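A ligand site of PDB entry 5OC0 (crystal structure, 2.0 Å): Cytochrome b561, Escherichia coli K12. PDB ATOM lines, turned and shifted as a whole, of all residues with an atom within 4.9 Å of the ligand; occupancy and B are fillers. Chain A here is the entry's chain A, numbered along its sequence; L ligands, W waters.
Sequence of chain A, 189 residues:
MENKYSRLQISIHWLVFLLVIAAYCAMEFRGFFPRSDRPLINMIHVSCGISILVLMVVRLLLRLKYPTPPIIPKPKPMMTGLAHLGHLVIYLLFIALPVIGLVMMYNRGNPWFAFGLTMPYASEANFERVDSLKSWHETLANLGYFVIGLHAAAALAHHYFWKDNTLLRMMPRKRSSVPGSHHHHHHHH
A ring nitrogen (NE2) of His 13 binds an iron atom (FE1) of the ligand (1.9 Å).
An iron atom (FE1) of the ligand is bound by a ring nitrogen (NE2) of His 151 (1.9 Å).
An oxygen (O3) of the ligand is in hydrogen-bond range of the side-chain hydroxyl (OH) of Tyr 91, at 2.6 Å.
The side-chain hydroxyl (OH) of Tyr 5 sits at hydrogen-bond distance from an oxygen (O1) of the ligand, 2.6 Å away.
The guanidinium group of Arg 169 is in salt-bridge range of an oxygen (O1) of the ligand, at 2.8 Å.
An oxygen (O4) of the ligand is in salt-bridge range of the guanidinium group (NH2) of Arg 59, 2.9 Å away.
NH2 of Arg 63 is in hydrogen-bond range of OH of Tyr 91, 2.8 Å away.
N of Tyr 5 sits at hydrogen-bond distance from O of Arg 169.
The backbone carbonyl oxygen of Thr 166 sits at hydrogen-bond distance from the guanidinium group of Arg 169.
The guanidinium group (NH1) of Arg 59 is in hydrogen-bond range of the side-chain sulfur (SD) of Met 56, at 3.5 Å.
The guanidinium group of Arg 63 lies within hydrogen-bond range of a ring nitrogen (ND1) of His 87, 3.2 Å away.
NH1 of Arg 63 is in hydrogen-bond range of OG1 of Thr 68 (3.1 Å).
NH1 of Arg 63 lies within hydrogen-bond range of NE2 of His 84 (3.3 Å).
NE1 of Trp 14 sits at hydrogen-bond distance from O of Met 170 (2.8 Å).
Trp 14 touches the ligand (CH2 to C14, 3.6 Å).
Phe 17 touches the ligand (CE1 to C18, 3.7 Å).
Val 20 touches the ligand (CG2 to C26, 3.98 Å).
Arg 63 touches the ligand (NH2 to C32, 3.4 Å).
CE1 of His 87 touches O2 of the ligand, 3.4 Å away.
CG2 of Ile 90 touches C4 of the ligand, at 3.8 Å.
Phe 94 touches the ligand.
Ile 148 touches the ligand (CG1 to C24, 3.9 Å).
CB of Ala 155 touches C2 of the ligand (3.7 Å).
O of Thr 166 touches C9 of the ligand, 3.6 Å away.
Leu 167 touches the ligand.
CE of Met 170 touches O4 of the ligand (3.5 Å).
Within 4 Å of the ligand: Tyr 5, His 13, Trp 14, Phe 17, Val 20, Arg 59, Arg 63, His 87, Ile 90, Tyr 91, Phe 94, Ile 148, His 151, Ala 155, Thr 166, Leu 167, Arg 169 and Met 170.
The nearest printed residue that does not touch the ligand is Ala 152 (4.1 Å).
Water W2 bridges an oxygen (O4) of the ligand (2.6 Å) and the backbone carbonyl oxygen of Gln 9 (2.9 Å).
Water W1 bridges an oxygen (O2) of the ligand (2.7 Å) and a ring nitrogen (NE2) of His 84 (2.8 Å).
Water W4 lies within hydrogen-bond range of the backbone carbonyl oxygen of His 13 (2.6 Å) and the guanidinium group of Arg 59 (2.8 Å).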
ATOM      1  N   TYR A   5      -3.765   1.134 -31.698  1.00  0.00           N
ATOM      2  CA  TYR A   5      -4.960   0.662 -30.996  1.00  0.00           C
ATOM      3  C   TYR A   5      -6.194   1.082 -31.787  1.00  0.00           C
ATOM      4  O   TYR A   5      -6.135   2.029 -32.561  1.00  0.00           O
ATOM      5  CB  TYR A   5      -5.027   1.285 -29.605  1.00  0.00           C
ATOM      6  CG  TYR A   5      -4.075   0.649 -28.636  1.00  0.00           C
ATOM      7  CD1 TYR A   5      -4.501  -0.405 -27.846  1.00  0.00           C
ATOM      8  CD2 TYR A   5      -2.773   1.156 -28.447  1.00  0.00           C
ATOM      9  CE1 TYR A   5      -3.622  -1.028 -26.953  1.00  0.00           C
ATOM     10  CE2 TYR A   5      -1.902   0.535 -27.565  1.00  0.00           C
ATOM     11  CZ  TYR A   5      -2.340  -0.525 -26.785  1.00  0.00           C
ATOM     12  OH  TYR A   5      -1.480  -1.110 -25.896  1.00  0.00           O
ATOM     13  N   GLN A   9     -10.530   2.137 -28.505  1.00  0.00           N
ATOM     14  CA  GLN A   9      -9.596   1.987 -27.379  1.00  0.00           C
ATOM     15  C   GLN A   9      -8.867   3.317 -27.124  1.00  0.00           C
ATOM     16  O   GLN A   9      -8.563   3.627 -25.970  1.00  0.00           O
ATOM     17  CB  GLN A   9      -8.580   0.911 -27.649  1.00  0.00           C
ATOM     18  CG  GLN A   9      -9.212  -0.500 -27.651  1.00  0.00           C
ATOM     19  CD  GLN A   9      -8.166  -1.557 -28.070  1.00  0.00           C
ATOM     20  OE1 GLN A   9      -7.680  -1.580 -29.236  1.00  0.00           O
ATOM     21  NE2 GLN A   9      -7.739  -2.330 -27.086  1.00  0.00           N
ATOM     22  N   HIS A  13      -9.061   5.433 -23.716  1.00  0.00           N
ATOM     23  CA  HIS A  13      -7.830   5.774 -23.043  1.00  0.00           C
ATOM     24  C   HIS A  13      -7.832   7.286 -22.593  1.00  0.00           C
ATOM     25  O   HIS A  13      -7.589   7.618 -21.395  1.00  0.00           O
ATOM     26  CB  HIS A  13      -6.554   5.433 -23.849  1.00  0.00           C
ATOM     27  CG  HIS A  13      -5.258   5.783 -23.161  1.00  0.00           C
ATOM     28  ND1 HIS A  13      -4.791   7.062 -23.125  1.00  0.00           N
ATOM     29  CD2 HIS A  13      -4.381   5.052 -22.404  1.00  0.00           C
ATOM     30  CE1 HIS A  13      -3.687   7.141 -22.389  1.00  0.00           C
ATOM     31  NE2 HIS A  13      -3.397   5.918 -21.936  1.00  0.00           N
ATOM     32  N   TRP A  14      -8.153   8.160 -23.544  1.00  0.00           N
ATOM     33  CA  TRP A  14      -8.009   9.575 -23.299  1.00  0.00           C
ATOM     34  C   TRP A  14      -9.245  10.112 -22.549  1.00  0.00           C
ATOM     35  O   TRP A  14      -9.119  11.049 -21.731  1.00  0.00           O
ATOM     36  CB  TRP A  14      -7.712  10.324 -24.607  1.00  0.00           C
ATOM     37  CG  TRP A  14      -6.384   9.940 -25.117  1.00  0.00           C
ATOM     38  CD1 TRP A  14      -6.112   9.177 -26.254  1.00  0.00           C
ATOM     39  CD2 TRP A  14      -5.129  10.155 -24.475  1.00  0.00           C
ATOM     40  NE1 TRP A  14      -4.760   8.973 -26.358  1.00  0.00           N
ATOM     41  CE2 TRP A  14      -4.125   9.601 -25.313  1.00  0.00           C
ATOM     42  CE3 TRP A  14      -4.744  10.881 -23.345  1.00  0.00           C
ATOM     43  CZ2 TRP A  14      -2.766   9.657 -24.998  1.00  0.00           C
ATOM     44  CZ3 TRP A  14      -3.413  10.895 -22.999  1.00  0.00           C
ATOM     45  CH2 TRP A  14      -2.430  10.285 -23.816  1.00  0.00           C
ATOM     46  N   VAL A  16     -10.791   8.367 -20.188  1.00  0.00           N
ATOM     47  CA  VAL A  16     -10.439   8.009 -18.827  1.00  0.00           C
ATOM     48  C   VAL A  16      -9.406   8.988 -18.230  1.00  0.00           C
ATOM     49  O   VAL A  16      -9.485   9.368 -17.039  1.00  0.00           O
ATOM     50  CB  VAL A  16      -9.990   6.566 -18.702  1.00  0.00           C
ATOM     51  CG1 VAL A  16      -9.311   6.253 -17.378  1.00  0.00           C
ATOM     52  CG2 VAL A  16     -11.184   5.610 -18.861  1.00  0.00           C
ATOM     53  N   PHE A  17      -8.400   9.323 -19.010  1.00  0.00           N
ATOM     54  CA  PHE A  17      -7.448  10.357 -18.593  1.00  0.00           C
ATOM     55  C   PHE A  17      -8.194  11.650 -18.141  1.00  0.00           C
ATOM     56  O   PHE A  17      -7.927  12.173 -17.061  1.00  0.00           O
ATOM     57  CB  PHE A  17      -6.474  10.643 -19.755  1.00  0.00           C
ATOM     58  CG  PHE A  17      -5.565  11.856 -19.580  1.00  0.00           C
ATOM     59  CD1 PHE A  17      -4.544  11.840 -18.665  1.00  0.00           C
ATOM     60  CD2 PHE A  17      -5.698  12.943 -20.396  1.00  0.00           C
ATOM     61  CE1 PHE A  17      -3.654  12.922 -18.536  1.00  0.00           C
ATOM     62  CE2 PHE A  17      -4.824  13.998 -20.317  1.00  0.00           C
ATOM     63  CZ  PHE A  17      -3.805  13.983 -19.372  1.00  0.00           C
ATOM     64  N   VAL A  20     -10.232  10.970 -14.916  1.00  0.00           N
ATOM     65  CA  VAL A  20      -9.327  10.830 -13.783  1.00  0.00           C
ATOM     66  C   VAL A  20      -8.830  12.192 -13.317  1.00  0.00           C
ATOM     67  O   VAL A  20      -8.724  12.434 -12.115  1.00  0.00           O
ATOM     68  CB  VAL A  20      -8.129   9.923 -14.127  1.00  0.00           C
ATOM     69  CG1 VAL A  20      -6.949  10.044 -13.155  1.00  0.00           C
ATOM     70  CG2 VAL A  20      -8.626   8.464 -14.166  1.00  0.00           C
ATOM     71  N   MET A  56     -12.782   1.245 -17.131  1.00  0.00           N
ATOM     72  CA  MET A  56     -11.664   0.411 -16.832  1.00  0.00           C
ATOM     73  C   MET A  56     -12.061  -1.077 -17.123  1.00  0.00           C
ATOM     74  O   MET A  56     -11.252  -1.833 -17.646  1.00  0.00           O
ATOM     75  CB  MET A  56     -11.216   0.572 -15.388  1.00  0.00           C
ATOM     76  CG  MET A  56     -10.612   1.916 -14.993  1.00  0.00           C
ATOM     77  SD  MET A  56      -9.042   2.380 -15.986  1.00  0.00           S
ATOM     78  CE  MET A  56      -7.917   0.824 -15.682  1.00  0.00           C
ATOM     79  N   ARG A  59     -12.493  -1.327 -21.062  1.00  0.00           N
ATOM     80  CA  ARG A  59     -11.215  -1.316 -21.735  1.00  0.00           C
ATOM     81  C   ARG A  59     -10.426  -2.621 -21.560  1.00  0.00           C
ATOM     82  O   ARG A  59      -9.672  -3.016 -22.425  1.00  0.00           O
ATOM     83  CB  ARG A  59     -10.383  -0.082 -21.347  1.00  0.00           C
ATOM     84  CG  ARG A  59      -9.594  -0.275 -20.070  1.00  0.00           C
ATOM     85  CD  ARG A  59      -9.080   1.040 -19.510  1.00  0.00           C
ATOM     86  NE  ARG A  59      -8.034   1.636 -20.319  1.00  0.00           N
ATOM     87  CZ  ARG A  59      -7.523   2.851 -20.086  1.00  0.00           C
ATOM     88  NH1 ARG A  59      -7.977   3.600 -19.084  1.00  0.00           N
ATOM     89  NH2 ARG A  59      -6.634   3.332 -20.883  1.00  0.00           N
ATOM     90  N   ARG A  63      -9.197  -5.135 -24.345  1.00  0.00           N
ATOM     91  CA  ARG A  63      -7.818  -5.547 -24.367  1.00  0.00           C
ATOM     92  C   ARG A  63      -7.690  -7.056 -24.565  1.00  0.00           C
ATOM     93  O   ARG A  63      -6.861  -7.516 -25.341  1.00  0.00           O
ATOM     94  CB  ARG A  63      -7.138  -4.972 -23.085  1.00  0.00           C
ATOM     95  CG  ARG A  63      -5.668  -4.973 -23.139  1.00  0.00           C
ATOM     96  CD  ARG A  63      -5.111  -3.989 -24.107  1.00  0.00           C
ATOM     97  NE  ARG A  63      -3.760  -4.331 -24.255  1.00  0.00           N
ATOM     98  CZ  ARG A  63      -2.788  -4.066 -23.367  1.00  0.00           C
ATOM     99  NH1 ARG A  63      -1.525  -4.423 -23.652  1.00  0.00           N
ATOM    100  NH2 ARG A  63      -3.033  -3.408 -22.213  1.00  0.00           N
ATOM    101  N   THR A  68      -2.794  -6.519 -28.994  1.00  0.00           N
ATOM    102  CA  THR A  68      -2.030  -5.307 -28.761  1.00  0.00           C
ATOM    103  C   THR A  68      -1.272  -4.896 -29.996  1.00  0.00           C
ATOM    104  O   THR A  68      -0.546  -5.655 -30.535  1.00  0.00           O
ATOM    105  CB  THR A  68      -1.109  -5.505 -27.554  1.00  0.00           C
ATOM    106  OG1 THR A  68      -1.940  -5.819 -26.429  1.00  0.00           O
ATOM    107  CG2 THR A  68      -0.271  -4.231 -27.197  1.00  0.00           C
ATOM    108  N   ILE A  71       4.909  -2.715 -31.199  1.00  0.00           N
ATOM    109  CA  ILE A  71       5.836  -1.585 -31.179  1.00  0.00           C
ATOM    110  C   ILE A  71       6.945  -1.767 -32.218  1.00  0.00           C
ATOM    111  O   ILE A  71       7.455  -2.867 -32.396  1.00  0.00           O
ATOM    112  CB  ILE A  71       6.371  -1.390 -29.741  1.00  0.00           C
ATOM    113  CG1 ILE A  71       5.157  -0.964 -28.843  1.00  0.00           C
ATOM    114  CG2 ILE A  71       7.446  -0.278 -29.669  1.00  0.00           C
ATOM    115  CD1 ILE A  71       5.425  -1.175 -27.405  1.00  0.00           C
ATOM    116  N   ALA A  83       5.946  -4.429 -19.535  1.00  0.00           N
ATOM    117  CA  ALA A  83       5.018  -3.374 -19.810  1.00  0.00           C
ATOM    118  C   ALA A  83       3.587  -3.934 -19.625  1.00  0.00           C
ATOM    119  O   ALA A  83       2.691  -3.265 -19.065  1.00  0.00           O
ATOM    120  CB  ALA A  83       5.231  -2.863 -21.214  1.00  0.00           C
ATOM    121  N   HIS A  84       3.343  -5.131 -20.149  1.00  0.00           N
ATOM    122  CA  HIS A  84       1.979  -5.758 -20.006  1.00  0.00           C
ATOM    123  C   HIS A  84       1.602  -6.021 -18.557  1.00  0.00           C
ATOM    124  O   HIS A  84       0.444  -5.773 -18.219  1.00  0.00           O
ATOM    125  CB  HIS A  84       1.706  -6.901 -21.028  1.00  0.00           C
ATOM    126  CG  HIS A  84       1.615  -6.349 -22.427  1.00  0.00           C
ATOM    127  ND1 HIS A  84       1.518  -7.132 -23.562  1.00  0.00           N
ATOM    128  CD2 HIS A  84       1.711  -5.047 -22.874  1.00  0.00           C
ATOM    129  CE1 HIS A  84       1.520  -6.372 -24.633  1.00  0.00           C
ATOM    130  NE2 HIS A  84       1.652  -5.108 -24.251  1.00  0.00           N
ATOM    131  N   HIS A  87       0.680  -2.711 -17.142  1.00  0.00           N
ATOM    132  CA  HIS A  87      -0.716  -2.459 -17.506  1.00  0.00           C
ATOM    133  C   HIS A  87      -1.682  -3.186 -16.563  1.00  0.00           C
ATOM    134  O   HIS A  87      -2.717  -2.630 -16.179  1.00  0.00           O
ATOM    135  CB  HIS A  87      -1.010  -2.853 -18.956  1.00  0.00           C
ATOM    136  CG  HIS A  87      -0.238  -2.050 -19.938  1.00  0.00           C
ATOM    137  ND1 HIS A  87      -0.106  -2.409 -21.266  1.00  0.00           N
ATOM    138  CD2 HIS A  87       0.439  -0.874 -19.800  1.00  0.00           C
ATOM    139  CE1 HIS A  87       0.654  -1.541 -21.890  1.00  0.00           C
ATOM    140  NE2 HIS A  87       0.983  -0.589 -21.026  1.00  0.00           N
ATOM    141  N   ILE A  90      -2.056  -1.290 -13.510  1.00  0.00           N
ATOM    142  CA  ILE A  90      -2.959  -0.147 -13.737  1.00  0.00           C
ATOM    143  C   ILE A  90      -4.432  -0.518 -13.755  1.00  0.00           C
ATOM    144  O   ILE A  90      -5.308   0.148 -13.083  1.00  0.00           O
ATOM    145  CB  ILE A  90      -2.582   0.659 -15.001  1.00  0.00           C
ATOM    146  CG1 ILE A  90      -1.201   1.308 -14.802  1.00  0.00           C
ATOM    147  CG2 ILE A  90      -3.573   1.758 -15.242  1.00  0.00           C
ATOM    148  CD1 ILE A  90      -0.527   1.642 -16.101  1.00  0.00           C
ATOM    149  N   TYR A  91      -4.732  -1.593 -14.480  1.00  0.00           N
ATOM    150  CA  TYR A  91      -6.120  -2.120 -14.505  1.00  0.00           C
ATOM    151  C   TYR A  91      -6.609  -2.409 -13.093  1.00  0.00           C
ATOM    152  O   TYR A  91      -7.696  -1.973 -12.708  1.00  0.00           O
ATOM    153  CB  TYR A  91      -6.244  -3.375 -15.378  1.00  0.00           C
ATOM    154  CG  TYR A  91      -6.029  -3.152 -16.828  1.00  0.00           C
ATOM    155  CD1 TYR A  91      -6.752  -2.208 -17.533  1.00  0.00           C
ATOM    156  CD2 TYR A  91      -5.104  -3.941 -17.561  1.00  0.00           C
ATOM    157  CE1 TYR A  91      -6.537  -2.025 -18.911  1.00  0.00           C
ATOM    158  CE2 TYR A  91      -4.893  -3.735 -18.920  1.00  0.00           C
ATOM    159  CZ  TYR A  91      -5.629  -2.786 -19.596  1.00  0.00           C
ATOM    160  OH  TYR A  91      -5.374  -2.574 -20.942  1.00  0.00           O
ATOM    161  N   PHE A  94      -6.899   0.968 -10.707  1.00  0.00           N
ATOM    162  CA  PHE A  94      -7.997   1.835 -11.107  1.00  0.00           C
ATOM    163  C   PHE A  94      -9.366   1.195 -11.184  1.00  0.00           C
ATOM    164  O   PHE A  94     -10.364   1.882 -11.497  1.00  0.00           O
ATOM    165  CB  PHE A  94      -7.601   2.604 -12.378  1.00  0.00           C
ATOM    166  CG  PHE A  94      -6.594   3.701 -12.090  1.00  0.00           C
ATOM    167  CD1 PHE A  94      -7.043   4.914 -11.591  1.00  0.00           C
ATOM    168  CD2 PHE A  94      -5.243   3.486 -12.224  1.00  0.00           C
ATOM    169  CE1 PHE A  94      -6.144   5.933 -11.237  1.00  0.00           C
ATOM    170  CE2 PHE A  94      -4.311   4.505 -11.877  1.00  0.00           C
ATOM    171  CZ  PHE A  94      -4.780   5.725 -11.371  1.00  0.00           C
ATOM    172  N   ILE A 148       0.460   6.707 -12.580  1.00  0.00           N
ATOM    173  CA  ILE A 148       0.221   7.494 -13.812  1.00  0.00           C
ATOM    174  C   ILE A 148       1.484   8.245 -14.220  1.00  0.00           C
ATOM    175  O   ILE A 148       1.803   8.290 -15.402  1.00  0.00           O
ATOM    176  CB  ILE A 148      -0.959   8.485 -13.681  1.00  0.00           C
ATOM    177  CG1 ILE A 148      -2.251   7.728 -13.536  1.00  0.00           C
ATOM    178  CG2 ILE A 148      -1.111   9.444 -14.864  1.00  0.00           C
ATOM    179  CD1 ILE A 148      -3.283   8.615 -12.887  1.00  0.00           C
ATOM    180  N   HIS A 151       3.906   5.824 -15.710  1.00  0.00           N
ATOM    181  CA  HIS A 151       3.286   5.377 -16.942  1.00  0.00           C
ATOM    182  C   HIS A 151       3.503   6.443 -18.051  1.00  0.00           C
ATOM    183  O   HIS A 151       3.939   6.100 -19.175  1.00  0.00           O
ATOM    184  CB  HIS A 151       1.800   5.101 -16.705  1.00  0.00           C
ATOM    185  CG  HIS A 151       0.982   4.850 -17.933  1.00  0.00           C
ATOM    186  ND1 HIS A 151       1.032   3.675 -18.676  1.00  0.00           N
ATOM    187  CD2 HIS A 151       0.044   5.606 -18.515  1.00  0.00           C
ATOM    188  CE1 HIS A 151       0.176   3.748 -19.671  1.00  0.00           C
ATOM    189  NE2 HIS A 151      -0.496   4.881 -19.578  1.00  0.00           N
ATOM    190  N   ALA A 152       3.195   7.709 -17.724  1.00  0.00           N
ATOM    191  CA  ALA A 152       3.263   8.808 -18.716  1.00  0.00           C
ATOM    192  C   ALA A 152       4.760   9.014 -19.089  1.00  0.00           C
ATOM    193  O   ALA A 152       5.099   9.243 -20.258  1.00  0.00           O
ATOM    194  CB  ALA A 152       2.671  10.082 -18.161  1.00  0.00           C
ATOM    195  N   ALA A 155       6.058   6.495 -21.497  1.00  0.00           N
ATOM    196  CA  ALA A 155       5.552   6.791 -22.796  1.00  0.00           C
ATOM    197  C   ALA A 155       6.378   7.879 -23.436  1.00  0.00           C
ATOM    198  O   ALA A 155       6.756   7.809 -24.638  1.00  0.00           O
ATOM    199  CB  ALA A 155       4.113   7.205 -22.699  1.00  0.00           C
ATOM    200  N   THR A 166       5.669   3.794 -29.673  1.00  0.00           N
ATOM    201  CA  THR A 166       4.840   3.427 -28.536  1.00  0.00           C
ATOM    202  C   THR A 166       3.694   4.324 -28.318  1.00  0.00           C
ATOM    203  O   THR A 166       2.550   3.863 -28.226  1.00  0.00           O
ATOM    204  CB  THR A 166       5.662   3.339 -27.232  1.00  0.00           C
ATOM    205  OG1 THR A 166       6.705   2.361 -27.444  1.00  0.00           O
ATOM    206  CG2 THR A 166       4.811   2.884 -26.072  1.00  0.00           C
ATOM    207  N   LEU A 167       3.965   5.628 -28.259  1.00  0.00           N
ATOM    208  CA  LEU A 167       2.890   6.607 -28.039  1.00  0.00           C
ATOM    209  C   LEU A 167       2.057   6.868 -29.273  1.00  0.00           C
ATOM    210  O   LEU A 167       0.881   7.097 -29.146  1.00  0.00           O
ATOM    211  CB  LEU A 167       3.424   7.926 -27.448  1.00  0.00           C
ATOM    212  CG  LEU A 167       2.493   9.129 -27.278  1.00  0.00           C
ATOM    213  CD1 LEU A 167       1.330   8.808 -26.370  1.00  0.00           C
ATOM    214  CD2 LEU A 167       3.225  10.410 -26.789  1.00  0.00           C
ATOM    215  N   ARG A 169       0.958   4.897 -31.404  1.00  0.00           N
ATOM    216  CA  ARG A 169      -0.070   3.821 -31.504  1.00  0.00           C
ATOM    217  C   ARG A 169      -1.343   4.171 -30.698  1.00  0.00           C
ATOM    218  O   ARG A 169      -2.452   3.585 -30.978  1.00  0.00           O
ATOM    219  CB  ARG A 169       0.504   2.512 -30.984  1.00  0.00           C
ATOM    220  CG  ARG A 169       1.611   1.879 -31.851  1.00  0.00           C
ATOM    221  CD  ARG A 169       2.619   1.159 -30.983  1.00  0.00           C
ATOM    222  NE  ARG A 169       2.051  -0.005 -30.219  1.00  0.00           N
ATOM    223  CZ  ARG A 169       1.730  -0.027 -28.938  1.00  0.00           C
ATOM    224  NH1 ARG A 169       1.915   1.068 -28.162  1.00  0.00           N
ATOM    225  NH2 ARG A 169       1.280  -1.150 -28.367  1.00  0.00           N
ATOM    226  N   MET A 170      -1.157   5.027 -29.680  1.00  0.00           N
ATOM    227  CA  MET A 170      -2.209   5.441 -28.738  1.00  0.00           C
ATOM    228  C   MET A 170      -2.733   6.833 -29.037  1.00  0.00           C
ATOM    229  O   MET A 170      -3.681   7.301 -28.321  1.00  0.00           O
ATOM    230  CB  MET A 170      -1.725   5.241 -27.305  1.00  0.00           C
ATOM    231  CG  MET A 170      -2.790   5.388 -26.181  1.00  0.00           C
ATOM    232  SD  MET A 170      -4.422   4.346 -26.511  1.00  0.00           S
ATOM    233  CE  MET A 170      -3.878   2.795 -25.439  1.00  0.00           C
HETATM  234  C1  LIG L   1      -1.741   2.539 -22.617  1.00  0.00           C
HETATM  235  C2  LIG L   1       0.439   6.844 -22.651  1.00  0.00           C
HETATM  236  C3  LIG L   1      -2.553   8.319 -19.142  1.00  0.00           C
HETATM  237  C4  LIG L   1      -3.846   3.754 -18.443  1.00  0.00           C
HETATM  238  C5  LIG L   1      -0.946   3.580 -22.975  1.00  0.00           C
HETATM  239  C6  LIG L   1       0.070   3.516 -23.957  1.00  0.00           C
HETATM  240  C7  LIG L   1       0.682   4.733 -23.987  1.00  0.00           C
HETATM  241  C8  LIG L   1       0.082   5.553 -22.989  1.00  0.00           C
HETATM  242  C9  LIG L   1       1.803   5.121 -24.891  1.00  0.00           C
HETATM  243  C10 LIG L   1       0.370   2.347 -24.841  1.00  0.00           C
HETATM  244  C11 LIG L   1       1.413   1.548 -24.077  1.00  0.00           C
HETATM  245  C12 LIG L   1       1.725   0.220 -24.782  1.00  0.00           C
HETATM  246  O1  LIG L   1       0.995  -0.214 -25.693  1.00  0.00           O
HETATM  247  O2  LIG L   1       2.693  -0.457 -24.452  1.00  0.00           O
HETATM  248  C13 LIG L   1      -0.176   7.668 -21.695  1.00  0.00           C
HETATM  249  C14 LIG L   1       0.114   9.096 -21.499  1.00  0.00           C
HETATM  250  C15 LIG L   1      -0.733   9.504 -20.491  1.00  0.00           C
HETATM  251  C16 LIG L   1      -1.564   8.307 -20.098  1.00  0.00           C
HETATM  252  C17 LIG L   1       1.182   9.897 -22.237  1.00  0.00           C
HETATM  253  C18 LIG L   1      -0.931  10.833 -19.878  1.00  0.00           C
HETATM  254  C19 LIG L   1      -0.399  11.942 -20.351  1.00  0.00           C
HETATM  255  C20 LIG L   1      -3.195   7.251 -18.589  1.00  0.00           C
HETATM  256  C21 LIG L   1      -4.035   7.257 -17.441  1.00  0.00           C
HETATM  257  C22 LIG L   1      -4.372   5.896 -17.242  1.00  0.00           C
HETATM  258  C23 LIG L   1      -3.745   5.119 -18.269  1.00  0.00           C
HETATM  259  C24 LIG L   1      -4.474   8.442 -16.598  1.00  0.00           C
HETATM  260  C25 LIG L   1      -5.234   5.273 -16.235  1.00  0.00           C
HETATM  261  C26 LIG L   1      -5.812   5.853 -15.224  1.00  0.00           C
HETATM  262  C27 LIG L   1      -3.369   3.069 -19.567  1.00  0.00           C
HETATM  263  C28 LIG L   1      -3.694   1.632 -19.765  1.00  0.00           C
HETATM  264  C29 LIG L   1      -3.105   1.288 -20.937  1.00  0.00           C
HETATM  265  C30 LIG L   1      -2.453   2.524 -21.437  1.00  0.00           C
HETATM  266  C31 LIG L   1      -4.473   0.767 -18.821  1.00  0.00           C
HETATM  267  C32 LIG L   1      -3.123  -0.043 -21.638  1.00  0.00           C
HETATM  268  C33 LIG L   1      -4.063  -0.018 -22.828  1.00  0.00           C
HETATM  269  C34 LIG L   1      -5.483   0.394 -22.478  1.00  0.00           C
HETATM  270  O3  LIG L   1      -6.216  -0.289 -21.700  1.00  0.00           O
HETATM  271  O4  LIG L   1      -5.952   1.456 -22.978  1.00  0.00           O
HETATM  272  N1  LIG L   1      -0.885   4.831 -22.348  1.00  0.00           N
HETATM  273  N2  LIG L   1      -1.175   7.331 -20.894  1.00  0.00           N
HETATM  274  N3  LIG L   1      -3.049   5.963 -19.078  1.00  0.00           N
HETATM  275  N4  LIG L   1      -2.662   3.544 -20.589  1.00  0.00           N
HETATM  276 FE1  LIG L   1      -1.962   5.384 -20.752  1.00  0.00          FE
HETATM  277  O   HOH W   1       2.962  -2.973 -25.515  1.00  0.00           O
HETATM  278  O   HOH W   2      -8.309   1.443 -24.028  1.00  0.00           O
HETATM  279  O   HOH W   3       4.457   0.637 -22.989  1.00  0.00           O
HETATM  280  O   HOH W   4      -6.549   6.006 -19.618  1.00  0.00           O
